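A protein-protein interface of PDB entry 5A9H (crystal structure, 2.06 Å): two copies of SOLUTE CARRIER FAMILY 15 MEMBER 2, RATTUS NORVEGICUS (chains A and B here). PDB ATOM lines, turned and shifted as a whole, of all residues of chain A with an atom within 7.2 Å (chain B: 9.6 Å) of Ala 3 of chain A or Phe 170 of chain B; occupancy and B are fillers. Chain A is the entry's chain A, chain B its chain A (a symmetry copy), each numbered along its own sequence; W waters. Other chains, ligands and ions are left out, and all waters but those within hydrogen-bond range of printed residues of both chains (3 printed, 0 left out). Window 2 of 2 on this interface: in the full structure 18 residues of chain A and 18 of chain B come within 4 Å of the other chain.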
ATOM      1  N   MET A   1      19.100  -7.829   4.224  1.00  0.00           N
ATOM      2  CA  MET A   1      19.050  -9.284   4.028  1.00  0.00           C
ATOM      3  C   MET A   1      17.697  -9.683   3.386  1.00  0.00           C
ATOM      4  O   MET A   1      17.642  -9.813   2.170  1.00  0.00           O
ATOM      5  CB  MET A   1      19.346 -10.064   5.340  1.00  0.00           C
ATOM      6  CG  MET A   1      20.773  -9.935   5.882  1.00  0.00           C
ATOM      7  SD  MET A   1      22.059 -11.202   5.505  1.00  0.00           S
ATOM      8  CE  MET A   1      21.022 -12.623   5.015  1.00  0.00           C
ATOM      9  N   ALA A   2      16.612  -9.823   4.169  1.00  0.00           N
ATOM     10  CA  ALA A   2      15.299 -10.212   3.633  1.00  0.00           C
ATOM     11  C   ALA A   2      14.479  -9.025   3.081  1.00  0.00           C
ATOM     12  O   ALA A   2      14.493  -7.938   3.662  1.00  0.00           O
ATOM     13  CB  ALA A   2      14.491 -10.947   4.686  1.00  0.00           C
ATOM     14  N   ALA A   3      13.719  -9.266   1.998  1.00  0.00           N
ATOM     15  CA  ALA A   3      12.856  -8.259   1.377  1.00  0.00           C
ATOM     16  C   ALA A   3      11.583  -8.013   2.222  1.00  0.00           C
ATOM     17  O   ALA A   3      11.321  -8.729   3.187  1.00  0.00           O
ATOM     18  CB  ALA A   3      12.480  -8.707  -0.033  1.00  0.00           C
ATOM     19  N   SER A   4      10.800  -6.998   1.859  1.00  0.00           N
ATOM     20  CA  SER A   4       9.525  -6.690   2.508  1.00  0.00           C
ATOM     21  C   SER A   4       8.627  -7.971   2.553  1.00  0.00           C
ATOM     22  O   SER A   4       8.634  -8.791   1.626  1.00  0.00           O
ATOM     23  CB  SER A   4       8.827  -5.557   1.759  1.00  0.00           C
ATOM     24  OG  SER A   4       7.583  -5.208   2.340  1.00  0.00           O
ATOM     25  N   GLN A   5       7.938  -8.173   3.682  1.00  0.00           N
ATOM     26  CA  GLN A   5       7.077  -9.330   3.940  1.00  0.00           C
ATOM     27  C   GLN A   5       7.839 -10.685   3.814  1.00  0.00           C
ATOM     28  O   GLN A   5       7.243 -11.710   3.464  1.00  0.00           O
ATOM     29  CB  GLN A   5       5.786  -9.266   3.100  1.00  0.00           C
ATOM     30  CG  GLN A   5       4.867  -8.166   3.623  1.00  0.00           C
ATOM     31  CD  GLN A   5       3.513  -8.044   2.963  1.00  0.00           C
ATOM     32  OE1 GLN A   5       2.972  -8.985   2.372  1.00  0.00           O
ATOM     33  NE2 GLN A   5       2.906  -6.878   3.119  1.00  0.00           N
ATOM     34  N   GLU A   6       9.159 -10.680   4.135  1.00  0.00           N
ATOM     35  CA  GLU A   6      10.003 -11.895   4.143  1.00  0.00           C
ATOM     36  C   GLU A   6      10.882 -11.910   5.390  1.00  0.00           C
ATOM     37  O   GLU A   6      11.327 -10.849   5.855  1.00  0.00           O
ATOM     38  CB  GLU A   6      10.975 -11.945   2.946  1.00  0.00           C
ATOM     39  CG  GLU A   6      10.369 -12.153   1.580  1.00  0.00           C
ATOM     40  CD  GLU A   6      11.368 -12.706   0.580  1.00  0.00           C
ATOM     41  OE1 GLU A   6      12.353 -12.005   0.255  1.00  0.00           O
ATOM     42  OE2 GLU A   6      11.176 -13.858   0.137  1.00  0.00           O
ATOM     43  N   ILE A   7      11.223 -13.116   5.857  1.00  0.00           N
ATOM     44  CA  ILE A   7      12.166 -13.337   6.947  1.00  0.00           C
ATOM     45  C   ILE A   7      13.105 -14.459   6.574  1.00  0.00           C
ATOM     46  O   ILE A   7      12.804 -15.253   5.673  1.00  0.00           O
ATOM     47  CB  ILE A   7      11.497 -13.631   8.338  1.00  0.00           C
ATOM     48  CG1 ILE A   7      10.688 -14.977   8.321  1.00  0.00           C
ATOM     49  CG2 ILE A   7      10.673 -12.441   8.824  1.00  0.00           C
ATOM     50  CD1 ILE A   7      10.455 -15.647   9.681  1.00  0.00           C
ATOM     51  N   PHE A   8      14.234 -14.533   7.293  1.00  0.00           N
ATOM     52  CA  PHE A   8      15.134 -15.671   7.240  1.00  0.00           C
ATOM     53  C   PHE A   8      14.952 -16.437   8.533  1.00  0.00           C
ATOM     54  O   PHE A   8      14.716 -15.840   9.583  1.00  0.00           O
ATOM     55  CB  PHE A   8      16.592 -15.281   7.065  1.00  0.00           C
ATOM     56  CG  PHE A   8      16.957 -15.033   5.629  1.00  0.00           C
ATOM     57  CD1 PHE A   8      17.189 -16.097   4.758  1.00  0.00           C
ATOM     58  CD2 PHE A   8      17.044 -13.738   5.131  1.00  0.00           C
ATOM     59  CE1 PHE A   8      17.548 -15.868   3.429  1.00  0.00           C
ATOM     60  CE2 PHE A   8      17.395 -13.511   3.800  1.00  0.00           C
ATOM     61  CZ  PHE A   8      17.649 -14.579   2.958  1.00  0.00           C
ATOM     62  N   LYS A  47      14.099 -19.019   3.669  1.00  0.00           N
ATOM     63  CA  LYS A  47      13.386 -17.772   3.496  1.00  0.00           C
ATOM     64  C   LYS A  47      11.895 -18.092   3.607  1.00  0.00           C
ATOM     65  O   LYS A  47      11.417 -19.040   2.985  1.00  0.00           O
ATOM     66  CB  LYS A  47      13.697 -17.158   2.128  1.00  0.00           C
ATOM     67  CG  LYS A  47      14.150 -15.720   2.234  1.00  0.00           C
ATOM     68  CD  LYS A  47      14.111 -15.014   0.897  1.00  0.00           C
ATOM     69  CE  LYS A  47      15.361 -15.173   0.077  1.00  0.00           C
ATOM     70  NZ  LYS A  47      15.345 -14.237  -1.081  1.00  0.00           N
ATOM     71  N   LEU A  48      11.180 -17.332   4.439  1.00  0.00           N
ATOM     72  CA  LEU A  48       9.744 -17.480   4.658  1.00  0.00           C
ATOM     73  C   LEU A  48       9.020 -16.232   4.180  1.00  0.00           C
ATOM     74  O   LEU A  48       9.453 -15.118   4.485  1.00  0.00           O
ATOM     75  CB  LEU A  48       9.423 -17.715   6.152  1.00  0.00           C
ATOM     76  CG  LEU A  48       9.557 -19.179   6.646  1.00  0.00           C
ATOM     77  CD1 LEU A  48      11.021 -19.624   6.728  1.00  0.00           C
ATOM     78  CD2 LEU A  48       8.915 -19.372   8.014  1.00  0.00           C
ATOM     79  N   GLU A  76       8.952  -8.465   9.392  1.00  0.00           N
ATOM     80  CA  GLU A  76       9.604  -8.474   8.090  1.00  0.00           C
ATOM     81  C   GLU A  76      11.056  -7.956   8.127  1.00  0.00           C
ATOM     82  O   GLU A  76      11.400  -7.108   8.960  1.00  0.00           O
ATOM     83  CB  GLU A  76       8.775  -7.623   7.099  1.00  0.00           C
ATOM     84  CG  GLU A  76       8.692  -6.141   7.456  1.00  0.00           C
ATOM     85  CD  GLU A  76       8.125  -5.238   6.379  1.00  0.00           C
ATOM     86  OE1 GLU A  76       7.738  -5.756   5.306  1.00  0.00           O
ATOM     87  OE2 GLU A  76       8.044  -4.010   6.619  1.00  0.00           O
ATOM     88  N   LYS A  77      11.883  -8.436   7.182  1.00  0.00           N
ATOM     89  CA  LYS A  77      13.281  -8.021   6.979  1.00  0.00           C
ATOM     90  C   LYS A  77      14.169  -8.317   8.189  1.00  0.00           C
ATOM     91  O   LYS A  77      15.098  -7.567   8.488  1.00  0.00           O
ATOM     92  CB  LYS A  77      13.381  -6.528   6.573  1.00  0.00           C
ATOM     93  CG  LYS A  77      12.559  -6.101   5.369  1.00  0.00           C
ATOM     94  CD  LYS A  77      12.558  -4.586   5.266  1.00  0.00           C
ATOM     95  CE  LYS A  77      11.926  -4.074   4.001  1.00  0.00           C
ATOM     96  NZ  LYS A  77      11.813  -2.588   4.012  1.00  0.00           N
ATOM     97  N   ASN A  78      13.864  -9.394   8.896  1.00  0.00           N
ATOM     98  CA  ASN A  78      14.634  -9.845  10.045  1.00  0.00           C
ATOM     99  C   ASN A  78      15.012 -11.288   9.826  1.00  0.00           C
ATOM    100  O   ASN A  78      14.384 -11.986   9.019  1.00  0.00           O
ATOM    101  CB  ASN A  78      13.822  -9.740  11.329  1.00  0.00           C
ATOM    102  CG  ASN A  78      13.729  -8.354  11.887  1.00  0.00           C
ATOM    103  OD1 ASN A  78      14.727  -7.752  12.277  1.00  0.00           O
ATOM    104  ND2 ASN A  78      12.528  -7.839  11.979  1.00  0.00           N
ATOM    105  N   MET B   1      26.601  -9.964   1.807  1.00  0.00           N
ATOM    106  CA  MET B   1      25.938 -11.219   2.188  1.00  0.00           C
ATOM    107  C   MET B   1      26.944 -12.145   2.919  1.00  0.00           C
ATOM    108  O   MET B   1      26.968 -12.130   4.143  1.00  0.00           O
ATOM    109  CB  MET B   1      25.255 -11.913   0.976  1.00  0.00           C
ATOM    110  CG  MET B   1      24.057 -11.172   0.374  1.00  0.00           C
ATOM    111  SD  MET B   1      22.328 -11.588   0.866  1.00  0.00           S
ATOM    112  CE  MET B   1      22.553 -13.260   1.566  1.00  0.00           C
ATOM    113  N   LYS B 102      19.787  -5.276  -5.560  1.00  0.00           N
ATOM    114  CA  LYS B 102      18.471  -5.261  -4.931  1.00  0.00           C
ATOM    115  C   LYS B 102      17.490  -4.513  -5.867  1.00  0.00           C
ATOM    116  O   LYS B 102      17.782  -3.371  -6.225  1.00  0.00           O
ATOM    117  CB  LYS B 102      18.543  -4.531  -3.573  1.00  0.00           C
ATOM    118  CG  LYS B 102      19.445  -5.214  -2.544  1.00  0.00           C
ATOM    119  CD  LYS B 102      19.528  -4.447  -1.226  1.00  0.00           C
ATOM    120  CE  LYS B 102      20.399  -5.167  -0.220  1.00  0.00           C
ATOM    121  NZ  LYS B 102      20.478  -4.435   1.070  1.00  0.00           N
ATOM    122  N   PRO B 103      16.343  -5.120  -6.277  1.00  0.00           N
ATOM    123  CA  PRO B 103      15.383  -4.369  -7.116  1.00  0.00           C
ATOM    124  C   PRO B 103      14.863  -3.130  -6.392  1.00  0.00           C
ATOM    125  O   PRO B 103      14.692  -3.128  -5.169  1.00  0.00           O
ATOM    126  CB  PRO B 103      14.232  -5.372  -7.351  1.00  0.00           C
ATOM    127  CG  PRO B 103      14.802  -6.727  -6.977  1.00  0.00           C
ATOM    128  CD  PRO B 103      15.818  -6.456  -5.923  1.00  0.00           C
ATOM    129  N   ALA B 104      14.602  -2.072  -7.154  1.00  0.00           N
ATOM    130  CA  ALA B 104      14.025  -0.841  -6.616  1.00  0.00           C
ATOM    131  C   ALA B 104      12.656  -1.172  -6.061  1.00  0.00           C
ATOM    132  O   ALA B 104      12.082  -2.201  -6.453  1.00  0.00           O
ATOM    133  CB  ALA B 104      13.895   0.163  -7.743  1.00  0.00           C
ATOM    134  N   ASN B 105      12.117  -0.322  -5.164  1.00  0.00           N
ATOM    135  CA  ASN B 105      10.773  -0.489  -4.585  1.00  0.00           C
ATOM    136  C   ASN B 105       9.720  -0.584  -5.714  1.00  0.00           C
ATOM    137  O   ASN B 105       9.754   0.201  -6.667  1.00  0.00           O
ATOM    138  CB  ASN B 105      10.449   0.692  -3.667  1.00  0.00           C
ATOM    139  CG  ASN B 105       9.184   0.545  -2.844  1.00  0.00           C
ATOM    140  OD1 ASN B 105       8.859  -0.530  -2.313  1.00  0.00           O
ATOM    141  ND2 ASN B 105       8.467   1.648  -2.675  1.00  0.00           N
ATOM    142  N   GLY B 106       8.842  -1.577  -5.624  1.00  0.00           N
ATOM    143  CA  GLY B 106       7.808  -1.809  -6.630  1.00  0.00           C
ATOM    144  C   GLY B 106       8.263  -2.742  -7.732  1.00  0.00           C
ATOM    145  O   GLY B 106       7.449  -3.164  -8.555  1.00  0.00           O
ATOM    146  N   MET B 107       9.570  -3.087  -7.751  1.00  0.00           N
ATOM    147  CA  MET B 107      10.165  -3.971  -8.743  1.00  0.00           C
ATOM    148  C   MET B 107      10.585  -5.311  -8.145  1.00  0.00           C
ATOM    149  O   MET B 107      10.753  -5.454  -6.920  1.00  0.00           O
ATOM    150  CB  MET B 107      11.428  -3.348  -9.412  1.00  0.00           C
ATOM    151  CG  MET B 107      11.291  -1.903  -9.925  1.00  0.00           C
ATOM    152  SD  MET B 107      10.188  -1.750 -11.338  1.00  0.00           S
ATOM    153  CE  MET B 107      11.205  -2.429 -12.686  1.00  0.00           C
ATOM    154  N   ALA B 108      10.797  -6.276  -9.053  1.00  0.00           N
ATOM    155  CA  ALA B 108      11.350  -7.592  -8.805  1.00  0.00           C
ATOM    156  C   ALA B 108      12.395  -7.797  -9.902  1.00  0.00           C
ATOM    157  O   ALA B 108      12.445  -7.004 -10.847  1.00  0.00           O
ATOM    158  CB  ALA B 108      10.249  -8.656  -8.890  1.00  0.00           C
ATOM    159  N   ALA B 109      13.273  -8.786  -9.754  1.00  0.00           N
ATOM    160  CA  ALA B 109      14.274  -9.103 -10.786  1.00  0.00           C
ATOM    161  C   ALA B 109      14.080 -10.571 -11.173  1.00  0.00           C
ATOM    162  O   ALA B 109      13.632 -11.371 -10.348  1.00  0.00           O
ATOM    163  CB  ALA B 109      15.694  -8.861 -10.274  1.00  0.00           C
ATOM    164  N   THR B 143      14.950  -6.477 -14.564  1.00  0.00           N
ATOM    165  CA  THR B 143      14.088  -5.932 -13.511  1.00  0.00           C
ATOM    166  C   THR B 143      12.723  -5.711 -14.115  1.00  0.00           C
ATOM    167  O   THR B 143      12.632  -5.208 -15.237  1.00  0.00           O
ATOM    168  CB  THR B 143      14.694  -4.685 -12.846  1.00  0.00           C
ATOM    169  OG1 THR B 143      13.906  -4.359 -11.697  1.00  0.00           O
ATOM    170  CG2 THR B 143      14.772  -3.466 -13.783  1.00  0.00           C
ATOM    171  N   VAL B 144      11.667  -6.104 -13.404  1.00  0.00           N
ATOM    172  CA  VAL B 144      10.289  -5.988 -13.902  1.00  0.00           C
ATOM    173  C   VAL B 144       9.435  -5.473 -12.786  1.00  0.00           C
ATOM    174  O   VAL B 144       9.835  -5.545 -11.624  1.00  0.00           O
ATOM    175  CB  VAL B 144       9.710  -7.345 -14.459  1.00  0.00           C
ATOM    176  CG1 VAL B 144      10.449  -7.819 -15.718  1.00  0.00           C
ATOM    177  CG2 VAL B 144       9.697  -8.437 -13.397  1.00  0.00           C
ATOM    178  N   LEU B 145       8.243  -4.993 -13.111  1.00  0.00           N
ATOM    179  CA  LEU B 145       7.316  -4.598 -12.065  1.00  0.00           C
ATOM    180  C   LEU B 145       6.871  -5.828 -11.266  1.00  0.00           C
ATOM    181  O   LEU B 145       6.710  -6.901 -11.834  1.00  0.00           O
ATOM    182  CB  LEU B 145       6.061  -3.977 -12.693  1.00  0.00           C
ATOM    183  CG  LEU B 145       6.007  -2.458 -12.892  1.00  0.00           C
ATOM    184  CD1 LEU B 145       5.945  -1.716 -11.560  1.00  0.00           C
ATOM    185  CD2 LEU B 145       7.084  -1.985 -13.830  1.00  0.00           C
ATOM    186  N   ARG B 146       6.637  -5.656  -9.962  1.00  0.00           N
ATOM    187  CA  ARG B 146       6.025  -6.663  -9.102  1.00  0.00           C
ATOM    188  C   ARG B 146       4.578  -6.878  -9.672  1.00  0.00           C
ATOM    189  O   ARG B 146       3.991  -5.957 -10.254  1.00  0.00           O
ATOM    190  CB  ARG B 146       5.993  -6.128  -7.651  1.00  0.00           C
ATOM    191  CG  ARG B 146       5.128  -6.891  -6.651  1.00  0.00           C
ATOM    192  CD  ARG B 146       3.838  -6.175  -6.300  1.00  0.00           C
ATOM    193  NE  ARG B 146       2.654  -7.017  -6.491  1.00  0.00           N
ATOM    194  CZ  ARG B 146       1.587  -7.010  -5.696  1.00  0.00           C
ATOM    195  NH1 ARG B 146       1.551  -6.224  -4.626  1.00  0.00           N
ATOM    196  NH2 ARG B 146       0.554  -7.801  -5.955  1.00  0.00           N
ATOM    197  N   GLY B 147       4.068  -8.103  -9.567  1.00  0.00           N
ATOM    198  CA  GLY B 147       2.743  -8.441 -10.077  1.00  0.00           C
ATOM    199  C   GLY B 147       2.681  -9.816 -10.704  1.00  0.00           C
ATOM    200  O   GLY B 147       3.620 -10.603 -10.577  1.00  0.00           O
ATOM    201  N   LYS B 148       1.558 -10.117 -11.366  1.00  0.00           N
ATOM    202  CA  LYS B 148       1.290 -11.417 -11.974  1.00  0.00           C
ATOM    203  C   LYS B 148       1.590 -11.408 -13.455  1.00  0.00           C
ATOM    204  O   LYS B 148       1.153 -10.503 -14.159  1.00  0.00           O
ATOM    205  CB  LYS B 148      -0.179 -11.816 -11.750  1.00  0.00           C
ATOM    206  CG  LYS B 148      -0.609 -11.924 -10.293  1.00  0.00           C
ATOM    207  CD  LYS B 148      -2.102 -12.229 -10.218  1.00  0.00           C
ATOM    208  CE  LYS B 148      -2.682 -11.929  -8.855  1.00  0.00           C
ATOM    209  NZ  LYS B 148      -4.166 -11.800  -8.901  1.00  0.00           N
ATOM    210  N   GLN B 167       3.046 -15.031  -9.526  1.00  0.00           N
ATOM    211  CA  GLN B 167       3.151 -13.789  -8.771  1.00  0.00           C
ATOM    212  C   GLN B 167       4.621 -13.445  -8.453  1.00  0.00           C
ATOM    213  O   GLN B 167       5.335 -14.273  -7.874  1.00  0.00           O
ATOM    214  CB  GLN B 167       2.299 -13.920  -7.479  1.00  0.00           C
ATOM    215  CG  GLN B 167       2.356 -12.744  -6.492  1.00  0.00           C
ATOM    216  CD  GLN B 167       1.602 -11.531  -6.970  1.00  0.00           C
ATOM    217  OE1 GLN B 167       0.368 -11.519  -7.047  1.00  0.00           O
ATOM    218  NE2 GLN B 167       2.332 -10.474  -7.281  1.00  0.00           N
ATOM    219  N   LEU B 168       5.071 -12.241  -8.827  1.00  0.00           N
ATOM    220  CA  LEU B 168       6.443 -11.797  -8.492  1.00  0.00           C
ATOM    221  C   LEU B 168       6.329 -10.759  -7.392  1.00  0.00           C
ATOM    222  O   LEU B 168       5.705  -9.723  -7.621  1.00  0.00           O
ATOM    223  CB  LEU B 168       7.219 -11.226  -9.711  1.00  0.00           C
ATOM    224  CG  LEU B 168       7.180 -12.066 -11.018  1.00  0.00           C
ATOM    225  CD1 LEU B 168       7.965 -11.401 -12.097  1.00  0.00           C
ATOM    226  CD2 LEU B 168       7.656 -13.514 -10.807  1.00  0.00           C
ATOM    227  N   ASP B 169       6.899 -11.045  -6.201  1.00  0.00           N
ATOM    228  CA  ASP B 169       6.857 -10.163  -5.013  1.00  0.00           C
ATOM    229  C   ASP B 169       7.868  -9.034  -5.002  1.00  0.00           C
ATOM    230  O   ASP B 169       8.983  -9.174  -5.512  1.00  0.00           O
ATOM    231  CB  ASP B 169       7.007 -10.965  -3.712  1.00  0.00           C
ATOM    232  CG  ASP B 169       5.921 -12.005  -3.454  1.00  0.00           C
ATOM    233  OD1 ASP B 169       4.767 -11.791  -3.912  1.00  0.00           O
ATOM    234  OD2 ASP B 169       6.214 -13.012  -2.762  1.00  0.00           O
ATOM    235  N   PHE B 170       7.483  -7.927  -4.343  1.00  0.00           N
ATOM    236  CA  PHE B 170       8.311  -6.745  -4.143  1.00  0.00           C
ATOM    237  C   PHE B 170       9.694  -7.156  -3.569  1.00  0.00           C
ATOM    238  O   PHE B 170       9.762  -7.887  -2.585  1.00  0.00           O
ATOM    239  CB  PHE B 170       7.658  -5.781  -3.109  1.00  0.00           C
ATOM    240  CG  PHE B 170       6.332  -5.113  -3.397  1.00  0.00           C
ATOM    241  CD1 PHE B 170       6.231  -4.120  -4.369  1.00  0.00           C
ATOM    242  CD2 PHE B 170       5.225  -5.354  -2.589  1.00  0.00           C
ATOM    243  CE1 PHE B 170       5.018  -3.440  -4.584  1.00  0.00           C
ATOM    244  CE2 PHE B 170       4.011  -4.687  -2.809  1.00  0.00           C
ATOM    245  CZ  PHE B 170       3.917  -3.729  -3.799  1.00  0.00           C
ATOM    246  N   GLY B 171      10.747  -6.653  -4.201  1.00  0.00           N
ATOM    247  CA  GLY B 171      12.142  -6.756  -3.798  1.00  0.00           C
ATOM    248  C   GLY B 171      12.777  -8.112  -3.919  1.00  0.00           C
ATOM    249  O   GLY B 171      13.873  -8.320  -3.407  1.00  0.00           O
ATOM    250  N   THR B 172      12.127  -9.024  -4.629  1.00  0.00           N
ATOM    251  CA  THR B 172      12.608 -10.384  -4.749  1.00  0.00           C
ATOM    252  C   THR B 172      13.226 -10.635  -6.135  1.00  0.00           C
ATOM    253  O   THR B 172      12.743 -10.099  -7.111  1.00  0.00           O
ATOM    254  CB  THR B 172      11.445 -11.329  -4.418  1.00  0.00           C
ATOM    255  OG1 THR B 172      10.897 -10.990  -3.137  1.00  0.00           O
ATOM    256  CG2 THR B 172      11.835 -12.770  -4.455  1.00  0.00           C
ATOM    257  N   THR B 173      14.276 -11.480  -6.197  1.00  0.00           N
ATOM    258  CA  THR B 173      14.949 -11.883  -7.425  1.00  0.00           C
ATOM    259  C   THR B 173      14.644 -13.371  -7.647  1.00  0.00           C
ATOM    260  O   THR B 173      14.785 -14.190  -6.735  1.00  0.00           O
ATOM    261  CB  THR B 173      16.444 -11.554  -7.332  1.00  0.00           C
ATOM    262  OG1 THR B 173      16.570 -10.149  -7.167  1.00  0.00           O
ATOM    263  CG2 THR B 173      17.204 -11.981  -8.569  1.00  0.00           C
ATOM    264  N   TYR B 174      14.174 -13.694  -8.831  1.00  0.00           N
ATOM    265  CA  TYR B 174      13.740 -15.040  -9.176  1.00  0.00           C
ATOM    266  C   TYR B 174      14.569 -15.661 -10.254  1.00  0.00           C
ATOM    267  O   TYR B 174      15.018 -14.965 -11.163  1.00  0.00           O
ATOM    268  CB  TYR B 174      12.284 -15.013  -9.694  1.00  0.00           C
ATOM    269  CG  TYR B 174      11.294 -14.536  -8.666  1.00  0.00           C
ATOM    270  CD1 TYR B 174      10.719 -15.425  -7.758  1.00  0.00           C
ATOM    271  CD2 TYR B 174      10.987 -13.178  -8.542  1.00  0.00           C
ATOM    272  CE1 TYR B 174       9.817 -14.983  -6.792  1.00  0.00           C
ATOM    273  CE2 TYR B 174      10.117 -12.723  -7.561  1.00  0.00           C
ATOM    274  CZ  TYR B 174       9.514 -13.634  -6.704  1.00  0.00           C
ATOM    275  OH  TYR B 174       8.650 -13.192  -5.741  1.00  0.00           O
ATOM    276  N   GLU B 192      13.847 -18.856  -5.893  1.00  0.00           N
ATOM    277  CA  GLU B 192      14.173 -17.509  -5.446  1.00  0.00           C
ATOM    278  C   GLU B 192      15.626 -17.423  -5.036  1.00  0.00           C
ATOM    279  O   GLU B 192      16.094 -18.246  -4.239  1.00  0.00           O
ATOM    280  CB  GLU B 192      13.289 -17.097  -4.263  1.00  0.00           C
ATOM    281  CG  GLU B 192      11.823 -16.998  -4.621  1.00  0.00           C
ATOM    282  CD  GLU B 192      10.901 -16.644  -3.474  1.00  0.00           C
ATOM    283  OE1 GLU B 192      11.290 -15.814  -2.615  1.00  0.00           O
ATOM    284  OE2 GLU B 192       9.770 -17.184  -3.452  1.00  0.00           O
ATOM    285  N   ASP B 193      16.330 -16.392  -5.541  1.00  0.00           N
ATOM    286  CA  ASP B 193      17.733 -16.140  -5.168  1.00  0.00           C
ATOM    287  C   ASP B 193      17.720 -15.682  -3.706  1.00  0.00           C
ATOM    288  O   ASP B 193      16.761 -15.029  -3.296  1.00  0.00           O
ATOM    289  CB  ASP B 193      18.324 -15.015  -6.008  1.00  0.00           C
ATOM    290  CG  ASP B 193      18.580 -15.332  -7.471  1.00  0.00           C
ATOM    291  OD1 ASP B 193      17.931 -16.255  -8.001  1.00  0.00           O
ATOM    292  OD2 ASP B 193      19.378 -14.602  -8.104  1.00  0.00           O
ATOM    293  N   ILE B 194      18.760 -16.015  -2.926  1.00  0.00           N
ATOM    294  CA  ILE B 194      18.853 -15.646  -1.515  1.00  0.00           C
ATOM    295  C   ILE B 194      18.599 -14.146  -1.224  1.00  0.00           C
ATOM    296  O   ILE B 194      19.133 -13.299  -1.922  1.00  0.00           O
ATOM    297  CB  ILE B 194      20.194 -16.119  -0.909  1.00  0.00           C
ATOM    298  CG1 ILE B 194      20.157 -15.957   0.620  1.00  0.00           C
ATOM    299  CG2 ILE B 194      21.403 -15.425  -1.607  1.00  0.00           C
ATOM    300  CD1 ILE B 194      21.154 -16.727   1.398  1.00  0.00           C
HETATM  301  O   HOH W   1      15.331 -12.661  -3.820  1.00  0.00           O
HETATM  302  O   HOH W   2      18.803 -10.516  -0.357  1.00  0.00           O
HETATM  303  O   HOH W   3       6.006 -11.954   0.481  1.00  0.00           O
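NZ of Lys 47 of chain A lies within hydrogen-bond range of O of Asp 193 of chain B (2.7 Å).
The side-chain carboxylate (OE2) of Glu 6 of chain A sits close to the side-chain carboxylate (OE1) of Glu 192 of chain B (3.4 Å).
The side-chain carboxylate (OE1) of Glu 6 of chain A is in salt-bridge range of the side-chain amino group (NZ) of Lys 47 of chain A (3.96 Å).
N of Lys 77 of chain A sits at hydrogen-bond distance from O of Glu 6 of chain A, at 2.8 Å.
O of Asn 78 of chain A lies within hydrogen-bond range of N of Phe 8 of chain A, 3.1 Å away.
The backbone NH (N) of Gly 171 of chain B lies within hydrogen-bond range of the backbone carbonyl oxygen (O) of Met 107 of chain B (3.0 Å).
N of Ala 109 of chain B lies within hydrogen-bond range of O of Thr 172 of chain B (3.0 Å).
The backbone carbonyl oxygen of Thr 173 of chain B sits at hydrogen-bond distance from the backbone NH of Asp 193 of chain B, 2.9 Å away.
Among the printed residues, pairs that only touch across the chains: Lys 47 of chain A with Ile 194 of chain B (3.3 Å), Ala 3 of chain A with Gly 171 of chain B (3.7 Å), Phe 8 of chain A with Ile 194 of chain B (3.7 Å), Ala 3 of chain A with Phe 170 of chain B (3.8 Å), Met 1 of chain A with Met 1 of chain B (3.8 Å) and Glu 6 of chain A with Thr 172 of chain B (3.8 Å).
Ala 2 of chain A touches none of the printed residues of chain B.
Of chain B, only Phe 170 (3.8 Å) and Gly 171 (3.7 Å) come within 4 Å of Ala 3 of chain A.
Of the printed residues of chain B, Glu 6 of chain A touches Thr 172 (3.8 Å) and Glu 192 (3.4 Å).
Ala 109 of chain B touches none of the printed residues of chain A.
Asp 169 of chain B touches none of the printed residues of chain A.
Phe 170 of chain B touches just one residue of chain A: Ala 3.
Of the printed residues of chain A, Gly 171 of chain B touches Ala 3.
Of the printed residues of chain A, Thr 172 of chain B touches Glu 6.
Printed residues of chain A within 4 Å of Asp 193 of chain B: Lys 47 (2.7 Å).
The nearest residue of chain B that does not touch Ala 3 of chain A is Thr 172 of chain B (4.2 Å).
The nearest residue of chain A that does not touch Phe 170 of chain B is Ser 4 of chain A (4.5 Å).
The nearest printed residue of chain A that does not touch Met 1 of chain B is Phe 8 of chain A (5.3 Å).
Of the 26 printed residues of chain B, 7 touch a printed residue of chain A.
Hydrophobic or aromatic side chains of chain B within 4 Å of the printed part of chain A: Met 1 and Ile 194.
Of the 13 printed residues of chain A, 5 touch a printed residue of chain B.
Printed residues of chain A that touch a printed residue of chain B: Met 1, Ala 3, Glu 6, Phe 8 and Lys 47.
Hydrophobic or aromatic side chains of chain A within 4 Å of the printed part of chain B: Met 1, Ala 3 and Phe 8.
Met 1 of chain B touches its own counterpart, Met 1 of chain A.
Position printed for both chains: 1.
Of the 8 pairs that touch across the chains among the printed residues, 1 has its exchanged pair printed and touching as well.
Water W1 lies within hydrogen-bond range of O of Asp 193 of chain B (2.8 Å), N of Thr 173 of chain B (2.9 Å) and NZ of Lys 47 of chain A (3.2 Å).
Water W2 lies within hydrogen-bond range of O of Met 1 of chain A (2.9 Å) and O of Ile 194 of chain B (3.2 Å).
Water W3 lies within hydrogen-bond range of the backbone carbonyl oxygen (O) of Gln 5 of chain A (3.2 Å) and the side-chain carboxylate (OD2) of Asp 169 of chain B (3.4 Å).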
